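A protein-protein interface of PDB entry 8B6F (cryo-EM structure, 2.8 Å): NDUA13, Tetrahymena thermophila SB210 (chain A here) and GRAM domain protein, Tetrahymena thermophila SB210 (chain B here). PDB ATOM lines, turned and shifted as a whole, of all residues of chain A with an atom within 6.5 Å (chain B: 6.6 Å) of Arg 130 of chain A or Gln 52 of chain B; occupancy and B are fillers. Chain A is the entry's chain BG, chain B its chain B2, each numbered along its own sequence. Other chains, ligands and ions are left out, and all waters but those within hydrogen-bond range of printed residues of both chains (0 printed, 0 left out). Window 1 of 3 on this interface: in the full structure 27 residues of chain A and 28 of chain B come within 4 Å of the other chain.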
ATOM      1  N   TYR A 112     -15.966   3.251  19.129  1.00  0.00           N
ATOM      2  CA  TYR A 112     -16.282   3.589  17.745  1.00  0.00           C
ATOM      3  C   TYR A 112     -15.020   3.689  16.900  1.00  0.00           C
ATOM      4  O   TYR A 112     -14.978   3.185  15.772  1.00  0.00           O
ATOM      5  CB  TYR A 112     -17.061   4.905  17.682  1.00  0.00           C
ATOM      6  CG  TYR A 112     -18.449   4.863  18.286  1.00  0.00           C
ATOM      7  CD1 TYR A 112     -18.976   3.688  18.807  1.00  0.00           C
ATOM      8  CD2 TYR A 112     -19.239   6.004  18.320  1.00  0.00           C
ATOM      9  CE1 TYR A 112     -20.246   3.653  19.350  1.00  0.00           C
ATOM     10  CE2 TYR A 112     -20.510   5.980  18.861  1.00  0.00           C
ATOM     11  CZ  TYR A 112     -21.008   4.802  19.375  1.00  0.00           C
ATOM     12  OH  TYR A 112     -22.273   4.773  19.914  1.00  0.00           O
ATOM     13  N   GLN A 125     -13.865   9.098  10.805  1.00  0.00           N
ATOM     14  CA  GLN A 125     -14.129  10.500  11.109  1.00  0.00           C
ATOM     15  C   GLN A 125     -15.423  10.968  10.454  1.00  0.00           C
ATOM     16  O   GLN A 125     -16.228  11.666  11.080  1.00  0.00           O
ATOM     17  CB  GLN A 125     -12.948  11.361  10.658  1.00  0.00           C
ATOM     18  CG  GLN A 125     -12.926  12.765  11.252  1.00  0.00           C
ATOM     19  CD  GLN A 125     -13.884  13.719  10.565  1.00  0.00           C
ATOM     20  OE1 GLN A 125     -14.335  13.471   9.449  1.00  0.00           O
ATOM     21  NE2 GLN A 125     -14.196  14.824  11.234  1.00  0.00           N
ATOM     22  N   LYS A 126     -15.644  10.589   9.192  1.00  0.00           N
ATOM     23  CA  LYS A 126     -16.875  10.974   8.509  1.00  0.00           C
ATOM     24  C   LYS A 126     -18.094  10.369   9.190  1.00  0.00           C
ATOM     25  O   LYS A 126     -19.127  11.032   9.333  1.00  0.00           O
ATOM     26  CB  LYS A 126     -16.822  10.548   7.042  1.00  0.00           C
ATOM     27  CG  LYS A 126     -15.866  11.363   6.191  1.00  0.00           C
ATOM     28  CD  LYS A 126     -15.961  10.969   4.724  1.00  0.00           C
ATOM     29  CE  LYS A 126     -15.100  11.873   3.855  1.00  0.00           C
ATOM     30  NZ  LYS A 126     -15.229  11.548   2.408  1.00  0.00           N
ATOM     31  N   MET A 127     -18.000   9.105   9.605  1.00  0.00           N
ATOM     32  CA  MET A 127     -19.123   8.473  10.290  1.00  0.00           C
ATOM     33  C   MET A 127     -19.435   9.175  11.606  1.00  0.00           C
ATOM     34  O   MET A 127     -20.605   9.374  11.949  1.00  0.00           O
ATOM     35  CB  MET A 127     -18.821   6.995  10.537  1.00  0.00           C
ATOM     36  CG  MET A 127     -19.129   6.087   9.359  1.00  0.00           C
ATOM     37  SD  MET A 127     -20.892   6.001   9.006  1.00  0.00           S
ATOM     38  CE  MET A 127     -20.921   4.753   7.728  1.00  0.00           C
ATOM     39  N   GLN A 128     -18.401   9.556  12.358  1.00  0.00           N
ATOM     40  CA  GLN A 128     -18.628  10.149  13.672  1.00  0.00           C
ATOM     41  C   GLN A 128     -19.140  11.581  13.563  1.00  0.00           C
ATOM     42  O   GLN A 128     -20.004  11.994  14.345  1.00  0.00           O
ATOM     43  CB  GLN A 128     -17.343  10.092  14.496  1.00  0.00           C
ATOM     44  CG  GLN A 128     -16.955   8.678  14.908  1.00  0.00           C
ATOM     45  CD  GLN A 128     -15.705   8.643  15.764  1.00  0.00           C
ATOM     46  OE1 GLN A 128     -15.143   9.681  16.106  1.00  0.00           O
ATOM     47  NE2 GLN A 128     -15.264   7.440  16.113  1.00  0.00           N
ATOM     48  N   LYS A 129     -18.627  12.355  12.608  1.00  0.00           N
ATOM     49  CA  LYS A 129     -19.060  13.740  12.470  1.00  0.00           C
ATOM     50  C   LYS A 129     -20.544  13.803  12.133  1.00  0.00           C
ATOM     51  O   LYS A 129     -21.040  13.048  11.293  1.00  0.00           O
ATOM     52  CB  LYS A 129     -18.246  14.446  11.386  1.00  0.00           C
ATOM     53  CG  LYS A 129     -18.575  15.925  11.241  1.00  0.00           C
ATOM     54  CD  LYS A 129     -17.678  16.602  10.219  1.00  0.00           C
ATOM     55  CE  LYS A 129     -18.042  18.068  10.049  1.00  0.00           C
ATOM     56  NZ  LYS A 129     -17.931  18.828  11.324  1.00  0.00           N
ATOM     57  N   ARG A 130     -21.256  14.722  12.788  1.00  0.00           N
ATOM     58  CA  ARG A 130     -22.704  14.802  12.646  1.00  0.00           C
ATOM     59  C   ARG A 130     -23.172  16.209  12.293  1.00  0.00           C
ATOM     60  O   ARG A 130     -24.198  16.371  11.627  1.00  0.00           O
ATOM     61  CB  ARG A 130     -23.381  14.327  13.934  1.00  0.00           C
ATOM     62  CG  ARG A 130     -24.869  14.045  13.783  1.00  0.00           C
ATOM     63  CD  ARG A 130     -25.362  13.078  14.851  1.00  0.00           C
ATOM     64  NE  ARG A 130     -25.467  13.698  16.167  1.00  0.00           N
ATOM     65  CZ  ARG A 130     -26.574  14.228  16.670  1.00  0.00           C
ATOM     66  NH1 ARG A 130     -27.705  14.254  15.984  1.00  0.00           N
ATOM     67  NH2 ARG A 130     -26.546  14.741  17.897  1.00  0.00           N
ATOM     68  N   PHE A 131     -22.435  17.230  12.728  1.00  0.00           N
ATOM     69  CA  PHE A 131     -22.822  18.620  12.525  1.00  0.00           C
ATOM     70  C   PHE A 131     -21.690  19.400  11.875  1.00  0.00           C
ATOM     71  O   PHE A 131     -20.521  19.233  12.234  1.00  0.00           O
ATOM     72  CB  PHE A 131     -23.199  19.292  13.854  1.00  0.00           C
ATOM     73  CG  PHE A 131     -24.465  18.767  14.468  1.00  0.00           C
ATOM     74  CD1 PHE A 131     -25.601  18.573  13.699  1.00  0.00           C
ATOM     75  CD2 PHE A 131     -24.517  18.468  15.817  1.00  0.00           C
ATOM     76  CE1 PHE A 131     -26.762  18.092  14.265  1.00  0.00           C
ATOM     77  CE2 PHE A 131     -25.675  17.988  16.389  1.00  0.00           C
ATOM     78  CZ  PHE A 131     -26.799  17.800  15.612  1.00  0.00           C
ATOM     79  N   HIS A 132     -22.047  20.258  10.916  1.00  0.00           N
ATOM     80  CA  HIS A 132     -21.064  21.164  10.328  1.00  0.00           C
ATOM     81  C   HIS A 132     -20.588  22.188  11.350  1.00  0.00           C
ATOM     82  O   HIS A 132     -19.387  22.449  11.472  1.00  0.00           O
ATOM     83  CB  HIS A 132     -21.657  21.871   9.108  1.00  0.00           C
ATOM     84  CG  HIS A 132     -21.970  20.957   7.966  1.00  0.00           C
ATOM     85  ND1 HIS A 132     -20.992  20.352   7.206  1.00  0.00           N
ATOM     86  CD2 HIS A 132     -23.152  20.561   7.440  1.00  0.00           C
ATOM     87  CE1 HIS A 132     -21.559  19.615   6.268  1.00  0.00           C
ATOM     88  NE2 HIS A 132     -22.869  19.724   6.388  1.00  0.00           N
ATOM     89  N   TRP A 137     -24.974  22.037  21.048  1.00  0.00           N
ATOM     90  CA  TRP A 137     -24.970  20.676  21.569  1.00  0.00           C
ATOM     91  C   TRP A 137     -26.377  20.108  21.453  1.00  0.00           C
ATOM     92  O   TRP A 137     -27.312  20.623  22.074  1.00  0.00           O
ATOM     93  CB  TRP A 137     -24.491  20.645  23.019  1.00  0.00           C
ATOM     94  CG  TRP A 137     -24.265  19.264  23.554  1.00  0.00           C
ATOM     95  CD1 TRP A 137     -23.553  18.263  22.960  1.00  0.00           C
ATOM     96  CD2 TRP A 137     -24.736  18.737  24.800  1.00  0.00           C
ATOM     97  NE1 TRP A 137     -23.556  17.145  23.758  1.00  0.00           N
ATOM     98  CE2 TRP A 137     -24.275  17.409  24.893  1.00  0.00           C
ATOM     99  CE3 TRP A 137     -25.504  19.259  25.845  1.00  0.00           C
ATOM    100  CZ2 TRP A 137     -24.558  16.596  25.987  1.00  0.00           C
ATOM    101  CZ3 TRP A 137     -25.784  18.449  26.931  1.00  0.00           C
ATOM    102  CH2 TRP A 137     -25.313  17.132  26.994  1.00  0.00           C
ATOM    103  N   ALA A 138     -26.522  19.050  20.659  1.00  0.00           N
ATOM    104  CA  ALA A 138     -27.806  18.395  20.421  1.00  0.00           C
ATOM    105  C   ALA A 138     -27.636  16.903  20.668  1.00  0.00           C
ATOM    106  O   ALA A 138     -27.400  16.129  19.731  1.00  0.00           O
ATOM    107  CB  ALA A 138     -28.310  18.662  19.004  1.00  0.00           C
ATOM    108  N   PRO A 139     -27.746  16.463  21.920  1.00  0.00           N
ATOM    109  CA  PRO A 139     -27.582  15.035  22.208  1.00  0.00           C
ATOM    110  C   PRO A 139     -28.605  14.203  21.452  1.00  0.00           C
ATOM    111  O   PRO A 139     -29.754  14.609  21.274  1.00  0.00           O
ATOM    112  CB  PRO A 139     -27.799  14.946  23.723  1.00  0.00           C
ATOM    113  CG  PRO A 139     -27.678  16.331  24.230  1.00  0.00           C
ATOM    114  CD  PRO A 139     -28.094  17.233  23.124  1.00  0.00           C
ATOM    115  N   PHE A 140     -28.175  13.028  21.005  1.00  0.00           N
ATOM    116  CA  PHE A 140     -29.073  12.119  20.310  1.00  0.00           C
ATOM    117  C   PHE A 140     -29.978  11.409  21.308  1.00  0.00           C
ATOM    118  O   PHE A 140     -29.508  10.875  22.317  1.00  0.00           O
ATOM    119  CB  PHE A 140     -28.279  11.095  19.502  1.00  0.00           C
ATOM    120  CG  PHE A 140     -29.113   9.958  18.993  1.00  0.00           C
ATOM    121  CD1 PHE A 140     -29.893  10.108  17.861  1.00  0.00           C
ATOM    122  CD2 PHE A 140     -29.105   8.733  19.638  1.00  0.00           C
ATOM    123  CE1 PHE A 140     -30.659   9.062  17.387  1.00  0.00           C
ATOM    124  CE2 PHE A 140     -29.867   7.682  19.169  1.00  0.00           C
ATOM    125  CZ  PHE A 140     -30.645   7.847  18.042  1.00  0.00           C
ATOM    126  N   GLU B  41     -28.813  21.414   6.591  1.00  0.00           N
ATOM    127  CA  GLU B  41     -28.444  20.036   6.891  1.00  0.00           C
ATOM    128  C   GLU B  41     -28.257  19.837   8.388  1.00  0.00           C
ATOM    129  O   GLU B  41     -28.630  18.792   8.930  1.00  0.00           O
ATOM    130  CB  GLU B  41     -27.169  19.656   6.139  1.00  0.00           C
ATOM    131  CG  GLU B  41     -26.816  18.186   6.251  1.00  0.00           C
ATOM    132  CD  GLU B  41     -25.690  17.789   5.322  1.00  0.00           C
ATOM    133  OE1 GLU B  41     -25.155  18.676   4.626  1.00  0.00           O
ATOM    134  OE2 GLU B  41     -25.342  16.591   5.284  1.00  0.00           O
ATOM    135  N   ASP B  42     -27.678  20.822   9.074  1.00  0.00           N
ATOM    136  CA  ASP B  42     -27.543  20.715  10.521  1.00  0.00           C
ATOM    137  C   ASP B  42     -28.909  20.647  11.189  1.00  0.00           C
ATOM    138  O   ASP B  42     -29.118  19.847  12.107  1.00  0.00           O
ATOM    139  CB  ASP B  42     -26.745  21.899  11.065  1.00  0.00           C
ATOM    140  CG  ASP B  42     -25.303  21.882  10.614  1.00  0.00           C
ATOM    141  OD1 ASP B  42     -24.751  20.778  10.434  1.00  0.00           O
ATOM    142  OD2 ASP B  42     -24.721  22.973  10.442  1.00  0.00           O
ATOM    143  N   GLU B  45     -30.437  17.293  10.506  1.00  0.00           N
ATOM    144  CA  GLU B  45     -29.771  16.272  11.304  1.00  0.00           C
ATOM    145  C   GLU B  45     -30.260  16.306  12.743  1.00  0.00           C
ATOM    146  O   GLU B  45     -30.583  15.263  13.324  1.00  0.00           O
ATOM    147  CB  GLU B  45     -28.256  16.468  11.237  1.00  0.00           C
ATOM    148  CG  GLU B  45     -27.466  15.505  12.107  1.00  0.00           C
ATOM    149  CD  GLU B  45     -27.785  14.057  11.812  1.00  0.00           C
ATOM    150  OE1 GLU B  45     -28.272  13.768  10.700  1.00  0.00           O
ATOM    151  OE2 GLU B  45     -27.554  13.207  12.695  1.00  0.00           O
ATOM    152  N   CYS B  46     -30.324  17.495  13.342  1.00  0.00           N
ATOM    153  CA  CYS B  46     -30.830  17.589  14.704  1.00  0.00           C
ATOM    154  C   CYS B  46     -32.279  17.139  14.804  1.00  0.00           C
ATOM    155  O   CYS B  46     -32.719  16.740  15.887  1.00  0.00           O
ATOM    156  CB  CYS B  46     -30.700  19.026  15.210  1.00  0.00           C
ATOM    157  SG  CYS B  46     -30.965  19.208  16.983  1.00  0.00           S
ATOM    158  N   HIS B  47     -33.029  17.189  13.702  1.00  0.00           N
ATOM    159  CA  HIS B  47     -34.435  16.806  13.710  1.00  0.00           C
ATOM    160  C   HIS B  47     -34.634  15.311  13.491  1.00  0.00           C
ATOM    161  O   HIS B  47     -35.401  14.673  14.216  1.00  0.00           O
ATOM    162  CB  HIS B  47     -35.192  17.599  12.640  1.00  0.00           C
ATOM    163  CG  HIS B  47     -36.654  17.290  12.584  1.00  0.00           C
ATOM    164  ND1 HIS B  47     -37.506  17.528  13.642  1.00  0.00           N
ATOM    165  CD2 HIS B  47     -37.417  16.759  11.601  1.00  0.00           C
ATOM    166  CE1 HIS B  47     -38.730  17.159  13.310  1.00  0.00           C
ATOM    167  NE2 HIS B  47     -38.703  16.689  12.077  1.00  0.00           N
ATOM    168  N   ARG B  49     -31.916  12.799  12.882  1.00  0.00           N
ATOM    169  CA  ARG B  49     -30.869  11.957  13.454  1.00  0.00           C
ATOM    170  C   ARG B  49     -30.522  10.788  12.537  1.00  0.00           C
ATOM    171  O   ARG B  49     -30.189   9.699  13.006  1.00  0.00           O
ATOM    172  CB  ARG B  49     -31.258  11.449  14.847  1.00  0.00           C
ATOM    173  CG  ARG B  49     -31.412  12.560  15.871  1.00  0.00           C
ATOM    174  CD  ARG B  49     -32.470  12.233  16.907  1.00  0.00           C
ATOM    175  NE  ARG B  49     -33.819  12.350  16.365  1.00  0.00           N
ATOM    176  CZ  ARG B  49     -34.926  12.124  17.058  1.00  0.00           C
ATOM    177  NH1 ARG B  49     -34.884  11.760  18.328  1.00  0.00           N
ATOM    178  NH2 ARG B  49     -36.104  12.266  16.462  1.00  0.00           N
ATOM    179  N   LYS B  50     -30.584  11.012  11.225  1.00  0.00           N
ATOM    180  CA  LYS B  50     -30.256   9.959  10.270  1.00  0.00           C
ATOM    181  C   LYS B  50     -28.801   9.528  10.404  1.00  0.00           C
ATOM    182  O   LYS B  50     -28.495   8.331  10.374  1.00  0.00           O
ATOM    183  CB  LYS B  50     -30.544  10.436   8.848  1.00  0.00           C
ATOM    184  CG  LYS B  50     -30.172   9.441   7.755  1.00  0.00           C
ATOM    185  CD  LYS B  50     -30.283  10.081   6.382  1.00  0.00           C
ATOM    186  CE  LYS B  50     -29.743   9.167   5.296  1.00  0.00           C
ATOM    187  NZ  LYS B  50     -29.754   9.828   3.962  1.00  0.00           N
ATOM    188  N   LYS B  51     -27.888  10.490  10.552  1.00  0.00           N
ATOM    189  CA  LYS B  51     -26.469  10.160  10.602  1.00  0.00           C
ATOM    190  C   LYS B  51     -26.142   9.297  11.813  1.00  0.00           C
ATOM    191  O   LYS B  51     -25.329   8.370  11.721  1.00  0.00           O
ATOM    192  CB  LYS B  51     -25.636  11.440  10.606  1.00  0.00           C
ATOM    193  CG  LYS B  51     -25.784  12.258   9.335  1.00  0.00           C
ATOM    194  CD  LYS B  51     -24.844  13.450   9.331  1.00  0.00           C
ATOM    195  CE  LYS B  51     -24.930  14.210   8.017  1.00  0.00           C
ATOM    196  NZ  LYS B  51     -23.976  15.354   7.973  1.00  0.00           N
ATOM    197  N   GLN B  52     -26.754   9.587  12.961  1.00  0.00           N
ATOM    198  CA  GLN B  52     -26.517   8.761  14.138  1.00  0.00           C
ATOM    199  C   GLN B  52     -27.040   7.346  13.932  1.00  0.00           C
ATOM    200  O   GLN B  52     -26.410   6.375  14.369  1.00  0.00           O
ATOM    201  CB  GLN B  52     -27.164   9.389  15.367  1.00  0.00           C
ATOM    202  CG  GLN B  52     -26.768   8.716  16.669  1.00  0.00           C
ATOM    203  CD  GLN B  52     -25.308   8.903  17.008  1.00  0.00           C
ATOM    204  OE1 GLN B  52     -24.623   9.734  16.414  1.00  0.00           O
ATOM    205  NE2 GLN B  52     -24.821   8.132  17.973  1.00  0.00           N
ATOM    206  N   TYR B  53     -28.185   7.202  13.265  1.00  0.00           N
ATOM    207  CA  TYR B  53     -28.699   5.867  12.976  1.00  0.00           C
ATOM    208  C   TYR B  53     -27.756   5.109  12.052  1.00  0.00           C
ATOM    209  O   TYR B  53     -27.537   3.906  12.230  1.00  0.00           O
ATOM    210  CB  TYR B  53     -30.094   5.960  12.361  1.00  0.00           C
ATOM    211  CG  TYR B  53     -31.191   6.191  13.373  1.00  0.00           C
ATOM    212  CD1 TYR B  53     -31.523   5.212  14.299  1.00  0.00           C
ATOM    213  CD2 TYR B  53     -31.901   7.381  13.394  1.00  0.00           C
ATOM    214  CE1 TYR B  53     -32.527   5.417  15.222  1.00  0.00           C
ATOM    215  CE2 TYR B  53     -32.906   7.595  14.315  1.00  0.00           C
ATOM    216  CZ  TYR B  53     -33.215   6.609  15.226  1.00  0.00           C
ATOM    217  OH  TYR B  53     -34.216   6.814  16.144  1.00  0.00           O
ATOM    218  N   ALA B  54     -27.195   5.792  11.055  1.00  0.00           N
ATOM    219  CA  ALA B  54     -26.219   5.145  10.186  1.00  0.00           C
ATOM    220  C   ALA B  54     -24.991   4.713  10.977  1.00  0.00           C
ATOM    221  O   ALA B  54     -24.465   3.614  10.770  1.00  0.00           O
ATOM    222  CB  ALA B  54     -25.825   6.085   9.049  1.00  0.00           C
ATOM    223  N   LEU B  55     -24.516   5.569  11.883  1.00  0.00           N
ATOM    224  CA  LEU B  55     -23.385   5.200  12.726  1.00  0.00           C
ATOM    225  C   LEU B  55     -23.716   3.988  13.585  1.00  0.00           C
ATOM    226  O   LEU B  55     -22.888   3.085  13.743  1.00  0.00           O
ATOM    227  CB  LEU B  55     -22.977   6.384  13.601  1.00  0.00           C
ATOM    228  CG  LEU B  55     -21.927   6.099  14.676  1.00  0.00           C
ATOM    229  CD1 LEU B  55     -20.663   5.528  14.064  1.00  0.00           C
ATOM    230  CD2 LEU B  55     -21.618   7.361  15.457  1.00  0.00           C
ATOM    231  N   ASN B  56     -24.925   3.950  14.147  1.00  0.00           N
ATOM    232  CA  ASN B  56     -25.327   2.813  14.970  1.00  0.00           C
ATOM    233  C   ASN B  56     -25.399   1.538  14.142  1.00  0.00           C
ATOM    234  O   ASN B  56     -25.009   0.462  14.607  1.00  0.00           O
ATOM    235  CB  ASN B  56     -26.673   3.097  15.633  1.00  0.00           C
ATOM    236  CG  ASN B  56     -26.608   4.255  16.606  1.00  0.00           C
ATOM    237  OD1 ASN B  56     -25.551   4.562  17.152  1.00  0.00           O
ATOM    238  ND2 ASN B  56     -27.744   4.904  16.828  1.00  0.00           N
ATOM    239  N   TYR B  57     -25.896   1.640  12.910  1.00  0.00           N
ATOM    240  CA  TYR B  57     -25.933   0.481  12.026  1.00  0.00           C
ATOM    241  C   TYR B  57     -24.528  -0.040  11.758  1.00  0.00           C
ATOM    242  O   TYR B  57     -24.276  -1.249  11.821  1.00  0.00           O
ATOM    243  CB  TYR B  57     -26.638   0.858  10.722  1.00  0.00           C
ATOM    244  CG  TYR B  57     -26.667  -0.234   9.677  1.00  0.00           C
ATOM    245  CD1 TYR B  57     -27.675  -1.188   9.670  1.00  0.00           C
ATOM    246  CD2 TYR B  57     -25.703  -0.290   8.681  1.00  0.00           C
ATOM    247  CE1 TYR B  57     -27.712  -2.180   8.708  1.00  0.00           C
ATOM    248  CE2 TYR B  57     -25.730  -1.277   7.715  1.00  0.00           C
ATOM    249  CZ  TYR B  57     -26.737  -2.219   7.734  1.00  0.00           C
ATOM    250  OH  TYR B  57     -26.766  -3.201   6.773  1.00  0.00           O
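The side-chain carboxylate (OE1) of Glu 41 of chain B is in hydrogen-bond range of a ring nitrogen (NE2) of His 132 of chain A. The side-chain carboxylate of Asp 42 of chain B lies within hydrogen-bond range of the backbone NH of His 132 of chain A, at 2.8 Å. The side-chain carboxylate (OE2) of Glu 45 of chain B lies within salt-bridge range of the guanidinium group (NH1) of Arg 130 of chain A (3.5 Å).
OE2 of Glu 41 of chain B is in salt-bridge range of NZ of Lys 51 of chain B, 3.3 Å away. OE1 of Glu 45 of chain B lies close to N of Lys 51 of chain B, 3.3 Å away. The backbone carbonyl oxygen (O) of His 47 of chain B sits at hydrogen-bond distance from the guanidinium group (NH2) of Arg 49 of chain B (3.4 Å). The backbone carbonyl oxygen (O) of Gln 52 of chain B sits close to the side-chain amide nitrogen (ND2) of Asn 56 of chain B, 3.2 Å away. The side-chain amino group (NZ) of Lys 129 of chain A sits at hydrogen-bond distance from the backbone carbonyl oxygen (O) of Phe 131 of chain A. NH2 of Arg 130 of chain A is in hydrogen-bond range of O of Ala 138 of chain A (2.5 Å).
Tyr 112 of chain A touches Leu 55 of chain B (CE2 to CD2, 3.8 Å). O of Arg 130 of chain A touches CD of Lys 51 of chain B, 3.8 Å away. CD of Arg 130 of chain A touches OE1 of Gln 52 of chain B (3.8 Å). Phe 131 of chain A touches Asp 42 of chain B. Glu 45 of chain B touches Phe 131 of chain A (CG to CE1, 3.4 Å). Phe 131 of chain A touches Cys 46 of chain B (CE1 to N, 3.7 Å). CB of Ala 138 of chain A touches SG of Cys 46 of chain B, 3.4 Å away. Phe 140 of chain A touches Arg 49 of chain B. Gln 52 of chain B touches Phe 140 of chain A.
Lys 129 of chain A touches none of the printed residues of chain B. Of chain B, only Glu 45 (3.0 Å), Lys 51 (3.8 Å) and Gln 52 (3.8 Å) come within 4 Å of Arg 130 of chain A. Of the printed residues of chain B, His 132 of chain A touches Glu 41 and Asp 42. Printed residues of chain B within 4 Å of Ala 138 of chain A: Cys 46 (3.4 Å). Pro 139 of chain A touches none of the printed residues of chain B. Printed residues of chain A within 4 Å of Glu 45 of chain B: Arg 130 and Phe 131. Gln 52 of chain B touches just these residues of chain A: Arg 130 and Phe 140. Printed residues of chain A within 4 Å of Leu 55 of chain B: Tyr 112. The nearest residue of chain A that does not touch Gln 52 of chain B is Tyr 112 of chain A (4.6 Å). The nearest printed residue of chain A that does not touch Lys 51 of chain B is Lys 129 of chain A (4.3 Å).
Of the 13 printed residues of chain A, 6 touch a printed residue of chain B. Hydrophobic or aromatic side chains of chain A that line the printed part of chain B: Tyr 112, Phe 131, His 132, Ala 138 and Phe 140. Of the 14 printed residues of chain B, 8 touch a printed residue of chain A. Printed residues of chain B that touch a printed residue of chain A: Glu 41, Asp 42, Glu 45, Cys 46, Arg 49, Lys 51, Gln 52 and Leu 55. Hydrophobic or aromatic side chains of chain B that line the printed part of chain A: Leu 55. Among the printed residues, Asp or Glu carboxylates within 4 Å of a Lys or Arg side-chain nitrogen of the other chain: Arg 130 of chain A with Glu 45 of chain B (3.5 Å).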
